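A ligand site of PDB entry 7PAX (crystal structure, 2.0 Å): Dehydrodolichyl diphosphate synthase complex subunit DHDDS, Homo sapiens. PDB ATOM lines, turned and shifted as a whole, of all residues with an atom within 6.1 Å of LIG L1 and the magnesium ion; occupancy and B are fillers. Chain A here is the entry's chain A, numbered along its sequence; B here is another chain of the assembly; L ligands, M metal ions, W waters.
The guanidinium group (NH2) of Arg 216 of chain B lies within salt-bridge range of the side-chain carboxylate (OE2) of Glu 216 of chain A, at 2.9 Å.
The side-chain carboxylate of Glu 216 of chain A is in salt-bridge range of the guanidinium group of Arg 218 of chain A (3.3 Å).
The side-chain hydroxyl (OG) of Ser 214 of chain A is in hydrogen-bond range of the side-chain carboxylate (OD2) of Asp 41, at 3.2 Å.
NH2 of Arg 45 lies within hydrogen-bond range of OG of Ser 214 of chain A.
OE2 of Glu 214 of chain B is in salt-bridge range of NH1 of Arg 216 of chain B (3.0 Å).
OG of Ser 86 lies within hydrogen-bond range of N of Glu 88 (3.0 Å).
The backbone carbonyl oxygen (O) of Glu 214 of chain B sits at hydrogen-bond distance from the guanidinium group (NH1) of Arg 218 of chain A (2.9 Å).
The side-chain carboxylate (OD2) of Asp 41 lies within salt-bridge range of the guanidinium group (NH2) of Arg 45, 3.5 Å away.
NH2 of Arg 45 touches the magnesium ion (3.9 Å).
Of the 28 residues printed, 2 come within 4 Å of the magnesium ion.
Water W1 bridges O4 of LG2 L2 and NE of Arg 216 of chain B.
Water W4 lies within hydrogen-bond range of O6 of LIG L1 (2.6 Å), OXT of Lys 219 of chain B (2.9 Å) and NH2 of Arg 92 (3.1 Å).
The magnesium ion is bound by water W1 (2.0 Å), the side-chain carboxylate (OD1) of Asp 41 (2.1 Å), an oxygen (O6) of LG2 L2 (2.2 Å), water W5 (2.2 Å), an oxygen (O2) of LG2 L2 (2.2 Å) and an oxygen (O2) of LIG L1 (2.2 Å).
Merely in contact with LIG L1: Ala 84 (3.4 Å), Tyr 83 (3.5 Å), Phe 85 (3.5 Å), Ile 39 (3.7 Å), Arg 216 of chain B (3.7 Å), Ser 86 (3.8 Å) and Leu 186 of chain B (3.997 Å).
Hydrophobic or aromatic side chains within 4 Å of LIG L1: Ile 39, Tyr 83 and Leu 186 of chain B.
Of the 28 residues printed, 15 come within 4 Å of LIG L1.
The nearest printed residue that does not touch LIG L1 is Met 40 (4.001 Å).
O5 of LIG L1 is in salt-bridge range of NH2 of Arg 212, 3.3 Å away.
O5 of LIG L1 is in salt-bridge range of NH2 of Arg 218 of chain A.
The side-chain hydroxyl (OG) of Ser 220 lies within hydrogen-bond range of an oxygen (O7) of LIG L1 (2.7 Å).
N of Leu 217 of chain B lies within hydrogen-bond range of O6 of LIG L1.
The backbone NH (N) of Gly 218 of chain B sits at hydrogen-bond distance from an oxygen (O6) of LIG L1 (2.8 Å).
ND2 of Asn 89 sits at hydrogen-bond distance from O3 of LIG L1.
N of Arg 45 sits at hydrogen-bond distance from O5 of LG2 L2, 2.7 Å away.
O1 of LG2 L2 lies within salt-bridge range of NH1 of Arg 92 (2.7 Å).
NH2 of Arg 92 lies within salt-bridge range of O3 of LIG L1 (3.8 Å).
N of Arg 44 sits at hydrogen-bond distance from O3 of LG2 L2 (2.9 Å).
An oxygen (O4) of LG2 L2 is in salt-bridge range of the guanidinium group of Arg 44 (2.9 Å).
The backbone NH of Gly 42 sits close to a sulfur (S1) of LG2 L2, 3.4 Å away.
The guanidinium group of Arg 45 lies within salt-bridge range of an oxygen (O5) of LG2 L2, 2.8 Å away.
The backbone NH (N) of Asn 43 lies within hydrogen-bond range of an oxygen (O3) of LG2 L2 (3.2 Å).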
ATOM      1  N   ILE A  39      -6.834   2.722  -0.006  1.00  0.00           N
ATOM      2  CA  ILE A  39      -6.791   1.313  -0.375  1.00  0.00           C
ATOM      3  C   ILE A  39      -5.842   0.624   0.607  1.00  0.00           C
ATOM      4  O   ILE A  39      -4.616   0.768   0.503  1.00  0.00           O
ATOM      5  CB  ILE A  39      -6.329   1.104  -1.822  1.00  0.00           C
ATOM      6  CG1 ILE A  39      -7.313   1.779  -2.786  1.00  0.00           C
ATOM      7  CG2 ILE A  39      -6.222  -0.371  -2.146  1.00  0.00           C
ATOM      8  CD1 ILE A  39      -6.825   1.831  -4.223  1.00  0.00           C
ATOM      9  N   MET A  40      -6.409  -0.123   1.552  1.00  0.00           N
ATOM     10  CA  MET A  40      -5.667  -0.624   2.719  1.00  0.00           C
ATOM     11  C   MET A  40      -4.932  -1.923   2.384  1.00  0.00           C
ATOM     12  O   MET A  40      -5.273  -3.013   2.845  1.00  0.00           O
ATOM     13  CB  MET A  40      -6.615  -0.825   3.898  1.00  0.00           C
ATOM     14  CG  MET A  40      -7.416   0.417   4.249  1.00  0.00           C
ATOM     15  SD  MET A  40      -8.506   0.178   5.663  1.00  0.00           S
ATOM     16  CE  MET A  40      -9.598  -1.102   5.055  1.00  0.00           C
ATOM     17  N   ASP A  41      -3.859  -1.774   1.604  1.00  0.00           N
ATOM     18  CA  ASP A  41      -3.204  -2.903   0.958  1.00  0.00           C
ATOM     19  C   ASP A  41      -1.925  -3.307   1.687  1.00  0.00           C
ATOM     20  O   ASP A  41      -1.206  -2.460   2.208  1.00  0.00           O
ATOM     21  CB  ASP A  41      -2.867  -2.535  -0.495  1.00  0.00           C
ATOM     22  CG  ASP A  41      -2.673  -3.761  -1.369  1.00  0.00           C
ATOM     23  OD1 ASP A  41      -3.044  -4.868  -0.933  1.00  0.00           O
ATOM     24  OD2 ASP A  41      -2.141  -3.599  -2.493  1.00  0.00           O
ATOM     25  N   GLY A  42      -1.645  -4.612   1.691  1.00  0.00           N
ATOM     26  CA  GLY A  42      -0.422  -5.159   2.243  1.00  0.00           C
ATOM     27  C   GLY A  42      -0.574  -5.946   3.531  1.00  0.00           C
ATOM     28  O   GLY A  42       0.457  -6.314   4.122  1.00  0.00           O
ATOM     29  N   ASN A  43      -1.800  -6.229   3.983  1.00  0.00           N
ATOM     30  CA  ASN A  43      -2.016  -6.926   5.249  1.00  0.00           C
ATOM     31  C   ASN A  43      -1.314  -8.276   5.280  1.00  0.00           C
ATOM     32  O   ASN A  43      -0.728  -8.663   6.301  1.00  0.00           O
ATOM     33  CB  ASN A  43      -3.508  -7.128   5.492  1.00  0.00           C
ATOM     34  CG  ASN A  43      -4.244  -5.835   5.761  1.00  0.00           C
ATOM     35  OD1 ASN A  43      -3.644  -4.766   5.808  1.00  0.00           O
ATOM     36  ND2 ASN A  43      -5.566  -5.927   5.938  1.00  0.00           N
ATOM     37  N   ARG A  44      -1.397  -9.033   4.180  1.00  0.00           N
ATOM     38  CA  ARG A  44      -0.876 -10.401   4.191  1.00  0.00           C
ATOM     39  C   ARG A  44       0.653 -10.416   4.109  1.00  0.00           C
ATOM     40  O   ARG A  44       1.297 -11.263   4.747  1.00  0.00           O
ATOM     41  CB  ARG A  44      -1.495 -11.210   3.058  1.00  0.00           C
ATOM     42  CG  ARG A  44      -2.994 -11.389   3.170  1.00  0.00           C
ATOM     43  CD  ARG A  44      -3.505 -12.360   2.092  1.00  0.00           C
ATOM     44  NE  ARG A  44      -3.165 -11.914   0.746  1.00  0.00           N
ATOM     45  CZ  ARG A  44      -3.589 -12.494  -0.369  1.00  0.00           C
ATOM     46  NH1 ARG A  44      -4.380 -13.563  -0.299  1.00  0.00           N
ATOM     47  NH2 ARG A  44      -3.231 -12.027  -1.557  1.00  0.00           N
ATOM     48  N   ARG A  45       1.238  -9.518   3.328  1.00  0.00           N
ATOM     49  CA  ARG A  45       2.691  -9.411   3.333  1.00  0.00           C
ATOM     50  C   ARG A  45       3.194  -8.981   4.698  1.00  0.00           C
ATOM     51  O   ARG A  45       4.201  -9.501   5.185  1.00  0.00           O
ATOM     52  CB  ARG A  45       3.140  -8.426   2.245  1.00  0.00           C
ATOM     53  CG  ARG A  45       3.131  -9.019   0.832  1.00  0.00           C
ATOM     54  CD  ARG A  45       3.149  -7.928  -0.227  1.00  0.00           C
ATOM     55  NE  ARG A  45       1.839  -7.283  -0.404  1.00  0.00           N
ATOM     56  CZ  ARG A  45       1.644  -6.240  -1.207  1.00  0.00           C
ATOM     57  NH1 ARG A  45       2.657  -5.730  -1.892  1.00  0.00           N
ATOM     58  NH2 ARG A  45       0.426  -5.704  -1.334  1.00  0.00           N
ATOM     59  N   TYR A  83     -11.160   1.006   1.175  1.00  0.00           N
ATOM     60  CA  TYR A  83     -11.368  -0.266   0.484  1.00  0.00           C
ATOM     61  C   TYR A  83     -11.134  -1.378   1.493  1.00  0.00           C
ATOM     62  O   TYR A  83      -9.989  -1.631   1.887  1.00  0.00           O
ATOM     63  CB  TYR A  83     -10.443  -0.409  -0.724  1.00  0.00           C
ATOM     64  CG  TYR A  83     -11.025  -1.237  -1.865  1.00  0.00           C
ATOM     65  CD1 TYR A  83     -10.350  -1.355  -3.071  1.00  0.00           C
ATOM     66  CD2 TYR A  83     -12.244  -1.881  -1.734  1.00  0.00           C
ATOM     67  CE1 TYR A  83     -10.870  -2.091  -4.124  1.00  0.00           C
ATOM     68  CE2 TYR A  83     -12.780  -2.631  -2.795  1.00  0.00           C
ATOM     69  CZ  TYR A  83     -12.081  -2.723  -3.979  1.00  0.00           C
ATOM     70  OH  TYR A  83     -12.589  -3.452  -5.032  1.00  0.00           O
ATOM     71  N   ALA A  84     -12.209  -2.053   1.908  1.00  0.00           N
ATOM     72  CA  ALA A  84     -12.121  -3.105   2.913  1.00  0.00           C
ATOM     73  C   ALA A  84     -12.326  -4.502   2.354  1.00  0.00           C
ATOM     74  O   ALA A  84     -11.757  -5.458   2.884  1.00  0.00           O
ATOM     75  CB  ALA A  84     -13.155  -2.863   4.017  1.00  0.00           C
ATOM     76  N   PHE A  85     -13.123  -4.662   1.301  1.00  0.00           N
ATOM     77  CA  PHE A  85     -13.298  -5.984   0.703  1.00  0.00           C
ATOM     78  C   PHE A  85     -13.725  -5.840  -0.744  1.00  0.00           C
ATOM     79  O   PHE A  85     -14.769  -5.232  -1.023  1.00  0.00           O
ATOM     80  CB  PHE A  85     -14.313  -6.815   1.488  1.00  0.00           C
ATOM     81  CG  PHE A  85     -14.255  -8.279   1.170  1.00  0.00           C
ATOM     82  CD1 PHE A  85     -15.120  -8.845   0.256  1.00  0.00           C
ATOM     83  CD2 PHE A  85     -13.307  -9.087   1.792  1.00  0.00           C
ATOM     84  CE1 PHE A  85     -15.072 -10.191  -0.039  1.00  0.00           C
ATOM     85  CE2 PHE A  85     -13.250 -10.436   1.507  1.00  0.00           C
ATOM     86  CZ  PHE A  85     -14.120 -10.994   0.589  1.00  0.00           C
ATOM     87  N   SER A  86     -12.955  -6.401  -1.650  1.00  0.00           N
ATOM     88  CA  SER A  86     -13.293  -6.400  -3.059  1.00  0.00           C
ATOM     89  C   SER A  86     -14.141  -7.616  -3.394  1.00  0.00           C
ATOM     90  O   SER A  86     -14.010  -8.685  -2.776  1.00  0.00           O
ATOM     91  CB  SER A  86     -12.033  -6.404  -3.925  1.00  0.00           C
ATOM     92  OG  SER A  86     -12.378  -6.528  -5.298  1.00  0.00           O
ATOM     93  N   GLU A  88     -13.529  -9.184  -5.938  1.00  0.00           N
ATOM     94  CA  GLU A  88     -12.479 -10.097  -6.371  1.00  0.00           C
ATOM     95  C   GLU A  88     -11.920 -10.917  -5.214  1.00  0.00           C
ATOM     96  O   GLU A  88     -11.456 -12.041  -5.416  1.00  0.00           O
ATOM     97  CB  GLU A  88     -11.343  -9.321  -7.053  1.00  0.00           C
ATOM     98  CG  GLU A  88     -11.767  -8.351  -8.144  1.00  0.00           C
ATOM     99  CD  GLU A  88     -12.314  -9.067  -9.387  1.00  0.00           C
ATOM    100  OE1 GLU A  88     -12.180 -10.304  -9.480  1.00  0.00           O
ATOM    101  OE2 GLU A  88     -12.871  -8.383 -10.271  1.00  0.00           O
ATOM    102  N   ASN A  89     -11.958 -10.376  -3.988  1.00  0.00           N
ATOM    103  CA  ASN A  89     -11.442 -11.090  -2.822  1.00  0.00           C
ATOM    104  C   ASN A  89     -12.274 -12.310  -2.456  1.00  0.00           C
ATOM    105  O   ASN A  89     -11.821 -13.136  -1.661  1.00  0.00           O
ATOM    106  CB  ASN A  89     -11.354 -10.154  -1.615  1.00  0.00           C
ATOM    107  CG  ASN A  89     -10.374  -9.023  -1.823  1.00  0.00           C
ATOM    108  OD1 ASN A  89     -10.608  -7.900  -1.385  1.00  0.00           O
ATOM    109  ND2 ASN A  89      -9.267  -9.320  -2.493  1.00  0.00           N
ATOM    110  N   ARG A  92     -10.440 -15.697  -2.886  1.00  0.00           N
ATOM    111  CA  ARG A  92      -9.447 -16.224  -1.966  1.00  0.00           C
ATOM    112  C   ARG A  92      -9.973 -17.493  -1.299  1.00  0.00           C
ATOM    113  O   ARG A  92     -11.125 -17.883  -1.466  1.00  0.00           O
ATOM    114  CB  ARG A  92      -9.074 -15.165  -0.922  1.00  0.00           C
ATOM    115  CG  ARG A  92      -8.522 -13.889  -1.554  1.00  0.00           C
ATOM    116  CD  ARG A  92      -8.027 -12.887  -0.521  1.00  0.00           C
ATOM    117  NE  ARG A  92      -7.353 -11.746  -1.170  1.00  0.00           N
ATOM    118  CZ  ARG A  92      -6.660 -10.819  -0.527  1.00  0.00           C
ATOM    119  NH1 ARG A  92      -6.530 -10.866   0.789  1.00  0.00           N
ATOM    120  NH2 ARG A  92      -6.089  -9.830  -1.203  1.00  0.00           N
ATOM    121  N   CYS A 160     -16.015   0.356   1.955  1.00  0.00           N
ATOM    122  CA  CYS A 160     -16.298  -0.281   0.674  1.00  0.00           C
ATOM    123  C   CYS A 160     -16.122  -1.782   0.849  1.00  0.00           C
ATOM    124  O   CYS A 160     -14.998  -2.283   0.903  1.00  0.00           O
ATOM    125  CB  CYS A 160     -15.413   0.298  -0.425  1.00  0.00           C
ATOM    126  SG  CYS A 160     -15.944   1.966  -0.914  1.00  0.00           S
ATOM    127  N   ARG A 212      -2.895   4.491  -1.862  1.00  0.00           N
ATOM    128  CA  ARG A 212      -2.708   3.040  -1.836  1.00  0.00           C
ATOM    129  C   ARG A 212      -1.354   2.702  -1.223  1.00  0.00           C
ATOM    130  O   ARG A 212      -0.316   3.214  -1.667  1.00  0.00           O
ATOM    131  CB  ARG A 212      -2.821   2.397  -3.217  1.00  0.00           C
ATOM    132  CG  ARG A 212      -2.675   0.873  -3.133  1.00  0.00           C
ATOM    133  CD  ARG A 212      -3.124   0.163  -4.382  1.00  0.00           C
ATOM    134  NE  ARG A 212      -3.244  -1.273  -4.167  1.00  0.00           N
ATOM    135  CZ  ARG A 212      -3.979  -2.070  -4.938  1.00  0.00           C
ATOM    136  NH1 ARG A 212      -4.646  -1.556  -5.959  1.00  0.00           N
ATOM    137  NH2 ARG A 212      -4.063  -3.372  -4.671  1.00  0.00           N
ATOM    138  N   SER A 214       1.593  -0.281   0.154  1.00  0.00           N
ATOM    139  CA  SER A 214       2.344  -1.505  -0.124  1.00  0.00           C
ATOM    140  C   SER A 214       3.177  -1.405  -1.393  1.00  0.00           C
ATOM    141  O   SER A 214       3.876  -2.358  -1.724  1.00  0.00           O
ATOM    142  CB  SER A 214       1.459  -2.767  -0.209  1.00  0.00           C
ATOM    143  OG  SER A 214       0.854  -2.903  -1.486  1.00  0.00           O
ATOM    144  N   GLU A 216       2.146  -1.020  -4.608  1.00  0.00           N
ATOM    145  CA  GLU A 216       1.482  -1.300  -5.871  1.00  0.00           C
ATOM    146  C   GLU A 216       1.047   0.010  -6.521  1.00  0.00           C
ATOM    147  O   GLU A 216       0.595   0.936  -5.843  1.00  0.00           O
ATOM    148  CB  GLU A 216       0.264  -2.204  -5.651  1.00  0.00           C
ATOM    149  CG  GLU A 216       0.547  -3.451  -4.832  1.00  0.00           C
ATOM    150  CD  GLU A 216       1.578  -4.356  -5.463  1.00  0.00           C
ATOM    151  OE1 GLU A 216       1.721  -4.336  -6.707  1.00  0.00           O
ATOM    152  OE2 GLU A 216       2.256  -5.095  -4.720  1.00  0.00           O
ATOM    153  N   ARG A 218      -1.413   0.439  -8.888  1.00  0.00           N
ATOM    154  CA  ARG A 218      -2.655   0.180  -9.599  1.00  0.00           C
ATOM    155  C   ARG A 218      -3.806   0.545  -8.672  1.00  0.00           C
ATOM    156  O   ARG A 218      -3.628   0.724  -7.474  1.00  0.00           O
ATOM    157  CB  ARG A 218      -2.757  -1.286 -10.034  1.00  0.00           C
ATOM    158  CG  ARG A 218      -2.545  -2.284  -8.891  1.00  0.00           C
ATOM    159  CD  ARG A 218      -2.807  -3.708  -9.350  1.00  0.00           C
ATOM    160  NE  ARG A 218      -2.440  -4.708  -8.356  1.00  0.00           N
ATOM    161  CZ  ARG A 218      -1.261  -5.334  -8.318  1.00  0.00           C
ATOM    162  NH1 ARG A 218      -0.323  -5.051  -9.228  1.00  0.00           N
ATOM    163  NH2 ARG A 218      -1.015  -6.232  -7.380  1.00  0.00           N
ATOM    164  N   LEU A 219      -4.998   0.666  -9.259  1.00  0.00           N
ATOM    165  CA  LEU A 219      -6.189   1.072  -8.515  1.00  0.00           C
ATOM    166  C   LEU A 219      -7.059  -0.095  -8.069  1.00  0.00           C
ATOM    167  O   LEU A 219      -7.873   0.087  -7.164  1.00  0.00           O
ATOM    168  CB  LEU A 219      -7.038   2.038  -9.358  1.00  0.00           C
ATOM    169  CG  LEU A 219      -6.276   3.284  -9.818  1.00  0.00           C
ATOM    170  CD1 LEU A 219      -7.110   4.121 -10.793  1.00  0.00           C
ATOM    171  CD2 LEU A 219      -5.873   4.110  -8.610  1.00  0.00           C
ATOM    172  N   SER A 220      -6.889  -1.257  -8.694  1.00  0.00           N
ATOM    173  CA  SER A 220      -7.647  -2.482  -8.384  1.00  0.00           C
ATOM    174  C   SER A 220      -9.146  -2.190  -8.235  1.00  0.00           C
ATOM    175  O   SER A 220      -9.782  -2.570  -7.254  1.00  0.00           O
ATOM    176  CB  SER A 220      -7.102  -3.145  -7.120  1.00  0.00           C
ATOM    177  OG  SER A 220      -5.795  -3.681  -7.350  1.00  0.00           O
ATOM    178  N   LEU B 186      -7.171  -2.037 -13.533  1.00  0.00           N
ATOM    179  CA  LEU B 186      -5.974  -2.775 -13.166  1.00  0.00           C
ATOM    180  C   LEU B 186      -4.729  -2.296 -13.895  1.00  0.00           C
ATOM    181  O   LEU B 186      -3.674  -2.942 -13.792  1.00  0.00           O
ATOM    182  CB  LEU B 186      -6.168  -4.273 -13.417  1.00  0.00           C
ATOM    183  CG  LEU B 186      -7.146  -4.957 -12.447  1.00  0.00           C
ATOM    184  CD1 LEU B 186      -7.477  -6.379 -12.895  1.00  0.00           C
ATOM    185  CD2 LEU B 186      -6.566  -4.953 -11.044  1.00  0.00           C
ATOM    186  N   GLU B 214       3.825  -7.506  -9.950  1.00  0.00           N
ATOM    187  CA  GLU B 214       3.107  -8.719  -9.587  1.00  0.00           C
ATOM    188  C   GLU B 214       1.618  -8.395  -9.544  1.00  0.00           C
ATOM    189  O   GLU B 214       1.185  -7.504  -8.804  1.00  0.00           O
ATOM    190  CB  GLU B 214       3.596  -9.252  -8.240  1.00  0.00           C
ATOM    191  CG  GLU B 214       3.071 -10.620  -7.893  1.00  0.00           C
ATOM    192  CD  GLU B 214       3.589 -11.105  -6.561  1.00  0.00           C
ATOM    193  OE1 GLU B 214       4.802 -10.937  -6.302  1.00  0.00           O
ATOM    194  OE2 GLU B 214       2.782 -11.643  -5.774  1.00  0.00           O
ATOM    195  N   GLN B 215       0.840  -9.121 -10.348  1.00  0.00           N
ATOM    196  CA  GLN B 215      -0.594  -8.907 -10.448  1.00  0.00           C
ATOM    197  C   GLN B 215      -1.291 -10.123  -9.849  1.00  0.00           C
ATOM    198  O   GLN B 215      -1.139 -11.245 -10.339  1.00  0.00           O
ATOM    199  CB  GLN B 215      -1.007  -8.680 -11.901  1.00  0.00           C
ATOM    200  CG  GLN B 215      -0.243  -7.536 -12.551  1.00  0.00           C
ATOM    201  CD  GLN B 215      -0.207  -7.623 -14.071  1.00  0.00           C
ATOM    202  OE1 GLN B 215       0.124  -8.660 -14.640  1.00  0.00           O
ATOM    203  NE2 GLN B 215      -0.552  -6.531 -14.737  1.00  0.00           N
ATOM    204  N   ARG B 216      -2.043  -9.899  -8.773  1.00  0.00           N
ATOM    205  CA  ARG B 216      -2.665 -10.997  -8.047  1.00  0.00           C
ATOM    206  C   ARG B 216      -4.159 -11.119  -8.302  1.00  0.00           C
ATOM    207  O   ARG B 216      -4.734 -12.169  -7.991  1.00  0.00           O
ATOM    208  CB  ARG B 216      -2.403 -10.835  -6.540  1.00  0.00           C
ATOM    209  CG  ARG B 216      -0.923 -10.963  -6.180  1.00  0.00           C
ATOM    210  CD  ARG B 216      -0.662 -10.747  -4.690  1.00  0.00           C
ATOM    211  NE  ARG B 216      -0.620  -9.336  -4.346  1.00  0.00           N
ATOM    212  CZ  ARG B 216       0.435  -8.550  -4.525  1.00  0.00           C
ATOM    213  NH1 ARG B 216       1.544  -9.045  -5.058  1.00  0.00           N
ATOM    214  NH2 ARG B 216       0.387  -7.276  -4.170  1.00  0.00           N
ATOM    215  N   LEU B 217      -4.803 -10.085  -8.838  1.00  0.00           N
ATOM    216  CA  LEU B 217      -6.208 -10.120  -9.265  1.00  0.00           C
ATOM    217  C   LEU B 217      -7.164 -10.411  -8.106  1.00  0.00           C
ATOM    218  O   LEU B 217      -8.239 -10.971  -8.306  1.00  0.00           O
ATOM    219  CB  LEU B 217      -6.408 -11.138 -10.391  1.00  0.00           C
ATOM    220  CG  LEU B 217      -5.403 -11.042 -11.546  1.00  0.00           C
ATOM    221  CD1 LEU B 217      -5.593 -12.197 -12.520  1.00  0.00           C
ATOM    222  CD2 LEU B 217      -5.528  -9.688 -12.235  1.00  0.00           C
ATOM    223  N   GLY B 218      -6.789 -10.016  -6.893  1.00  0.00           N
ATOM    224  CA  GLY B 218      -7.623 -10.221  -5.736  1.00  0.00           C
ATOM    225  C   GLY B 218      -7.343 -11.474  -4.953  1.00  0.00           C
ATOM    226  O   GLY B 218      -7.872 -11.626  -3.839  1.00  0.00           O
ATOM    227  N   LYS B 219      -6.530 -12.375  -5.483  1.00  0.00           N
ATOM    228  CA  LYS B 219      -6.224 -13.653  -4.839  1.00  0.00           C
ATOM    229  C   LYS B 219      -5.061 -13.546  -3.864  1.00  0.00           C
ATOM    230  O   LYS B 219      -4.888 -14.390  -2.985  1.00  0.00           O
ATOM    231  CB  LYS B 219      -5.916 -14.726  -5.883  1.00  0.00           C
ATOM    232  CG  LYS B 219      -7.088 -15.605  -6.232  1.00  0.00           C
ATOM    233  CD  LYS B 219      -6.873 -16.293  -7.573  1.00  0.00           C
ATOM    234  CE  LYS B 219      -7.365 -17.734  -7.530  1.00  0.00           C
ATOM    235  NZ  LYS B 219      -6.714 -18.582  -8.569  1.00  0.00           N
ATOM    236  OXT LYS B 219      -4.244 -12.633  -3.948  1.00  0.00           O
HETATM  237  C1  LIG L   1      -7.864  -4.291  -3.225  1.00  0.00           C
HETATM  238  O1  LIG L   1      -6.643  -4.914  -2.940  1.00  0.00           O
HETATM  239  C2  LIG L   1      -8.948  -4.845  -2.300  1.00  0.00           C
HETATM  240  C3  LIG L   1      -8.901  -4.232  -0.898  1.00  0.00           C
HETATM  241  C4  LIG L   1      -9.819  -4.557   0.007  1.00  0.00           C
HETATM  242  C5  LIG L   1      -7.786  -3.252  -0.527  1.00  0.00           C
HETATM  243  P1  LIG L   1      -6.194  -6.273  -3.729  1.00  0.00           P
HETATM  244  O2  LIG L   1      -5.005  -6.895  -3.079  1.00  0.00           O
HETATM  245  O3  LIG L   1      -7.338  -7.246  -3.698  1.00  0.00           O
HETATM  246  O4  LIG L   1      -5.782  -5.869  -5.257  1.00  0.00           O
HETATM  247  P2  LIG L   1      -4.703  -6.672  -6.190  1.00  0.00           P
HETATM  248  O5  LIG L   1      -3.280  -6.385  -5.814  1.00  0.00           O
HETATM  249  O6  LIG L   1      -4.936  -8.162  -6.049  1.00  0.00           O
HETATM  250  O7  LIG L   1      -4.959  -6.221  -7.611  1.00  0.00           O
HETATM  251  C1  LG2 L   2      -6.313  -5.695   1.655  1.00  0.00           C
HETATM  252  S1  LG2 L   2      -4.621  -6.093   2.185  1.00  0.00           S
HETATM  253  C2  LG2 L   2      -7.296  -5.813   2.815  1.00  0.00           C
HETATM  254  C3  LG2 L   2      -8.192  -6.770   2.853  1.00  0.00           C
HETATM  255  C4  LG2 L   2      -8.263  -7.806   1.736  1.00  0.00           C
HETATM  256  C5  LG2 L   2      -9.158  -6.864   4.040  1.00  0.00           C
HETATM  257  C6  LG2 L   2      -9.238  -5.493   4.724  1.00  0.00           C
HETATM  258  C7  LG2 L   2      -9.010  -5.659   6.224  1.00  0.00           C
HETATM  259  C8  LG2 L   2      -9.856  -5.176   7.112  1.00  0.00           C
HETATM  260  C9  LG2 L   2     -11.126  -4.425   6.706  1.00  0.00           C
HETATM  261  C10 LG2 L   2      -9.566  -5.383   8.580  1.00  0.00           C
HETATM  262  C11 LG2 L   2     -12.336  -5.328   6.919  1.00  0.00           C
HETATM  263  C12 LG2 L   2     -12.997  -5.115   8.283  1.00  0.00           C
HETATM  264  C13 LG2 L   2     -13.928  -4.205   8.473  1.00  0.00           C
HETATM  265  C14 LG2 L   2     -14.569  -4.038   9.848  1.00  0.00           C
HETATM  266  C15 LG2 L   2     -14.409  -3.287   7.345  1.00  0.00           C
HETATM  267  P1  LG2 L   2      -4.160  -7.976   1.340  1.00  0.00           P
HETATM  268  O1  LG2 L   2      -5.041  -9.016   1.988  1.00  0.00           O
HETATM  269  O2  LG2 L   2      -4.431  -7.904  -0.142  1.00  0.00           O
HETATM  270  O3  LG2 L   2      -2.588  -8.312   1.674  1.00  0.00           O
HETATM  271  P2  LG2 L   2      -1.408  -8.375   0.546  1.00  0.00           P
HETATM  272  O4  LG2 L   2      -1.528  -9.686  -0.209  1.00  0.00           O
HETATM  273  O5  LG2 L   2      -0.094  -8.333   1.267  1.00  0.00           O
HETATM  274  O6  LG2 L   2      -1.573  -7.217  -0.429  1.00  0.00           O
HETATM  275 MG    MG M   1      -3.300  -6.812  -1.649  1.00  0.00          MG
HETATM  276  O   HOH W   1      -2.944  -8.542  -2.516  1.00  0.00           O
HETATM  277  O   HOH W   2      -3.671  -7.612  -9.474  1.00  0.00           O
HETATM  278  O   HOH W   3      -7.532  -6.890  -8.408  1.00  0.00           O
HETATM  279  O   HOH W   4      -4.788  -9.782  -3.997  1.00  0.00           O
HETATM  280  O   HOH W   5      -2.282  -6.022  -3.382  1.00  0.00           O
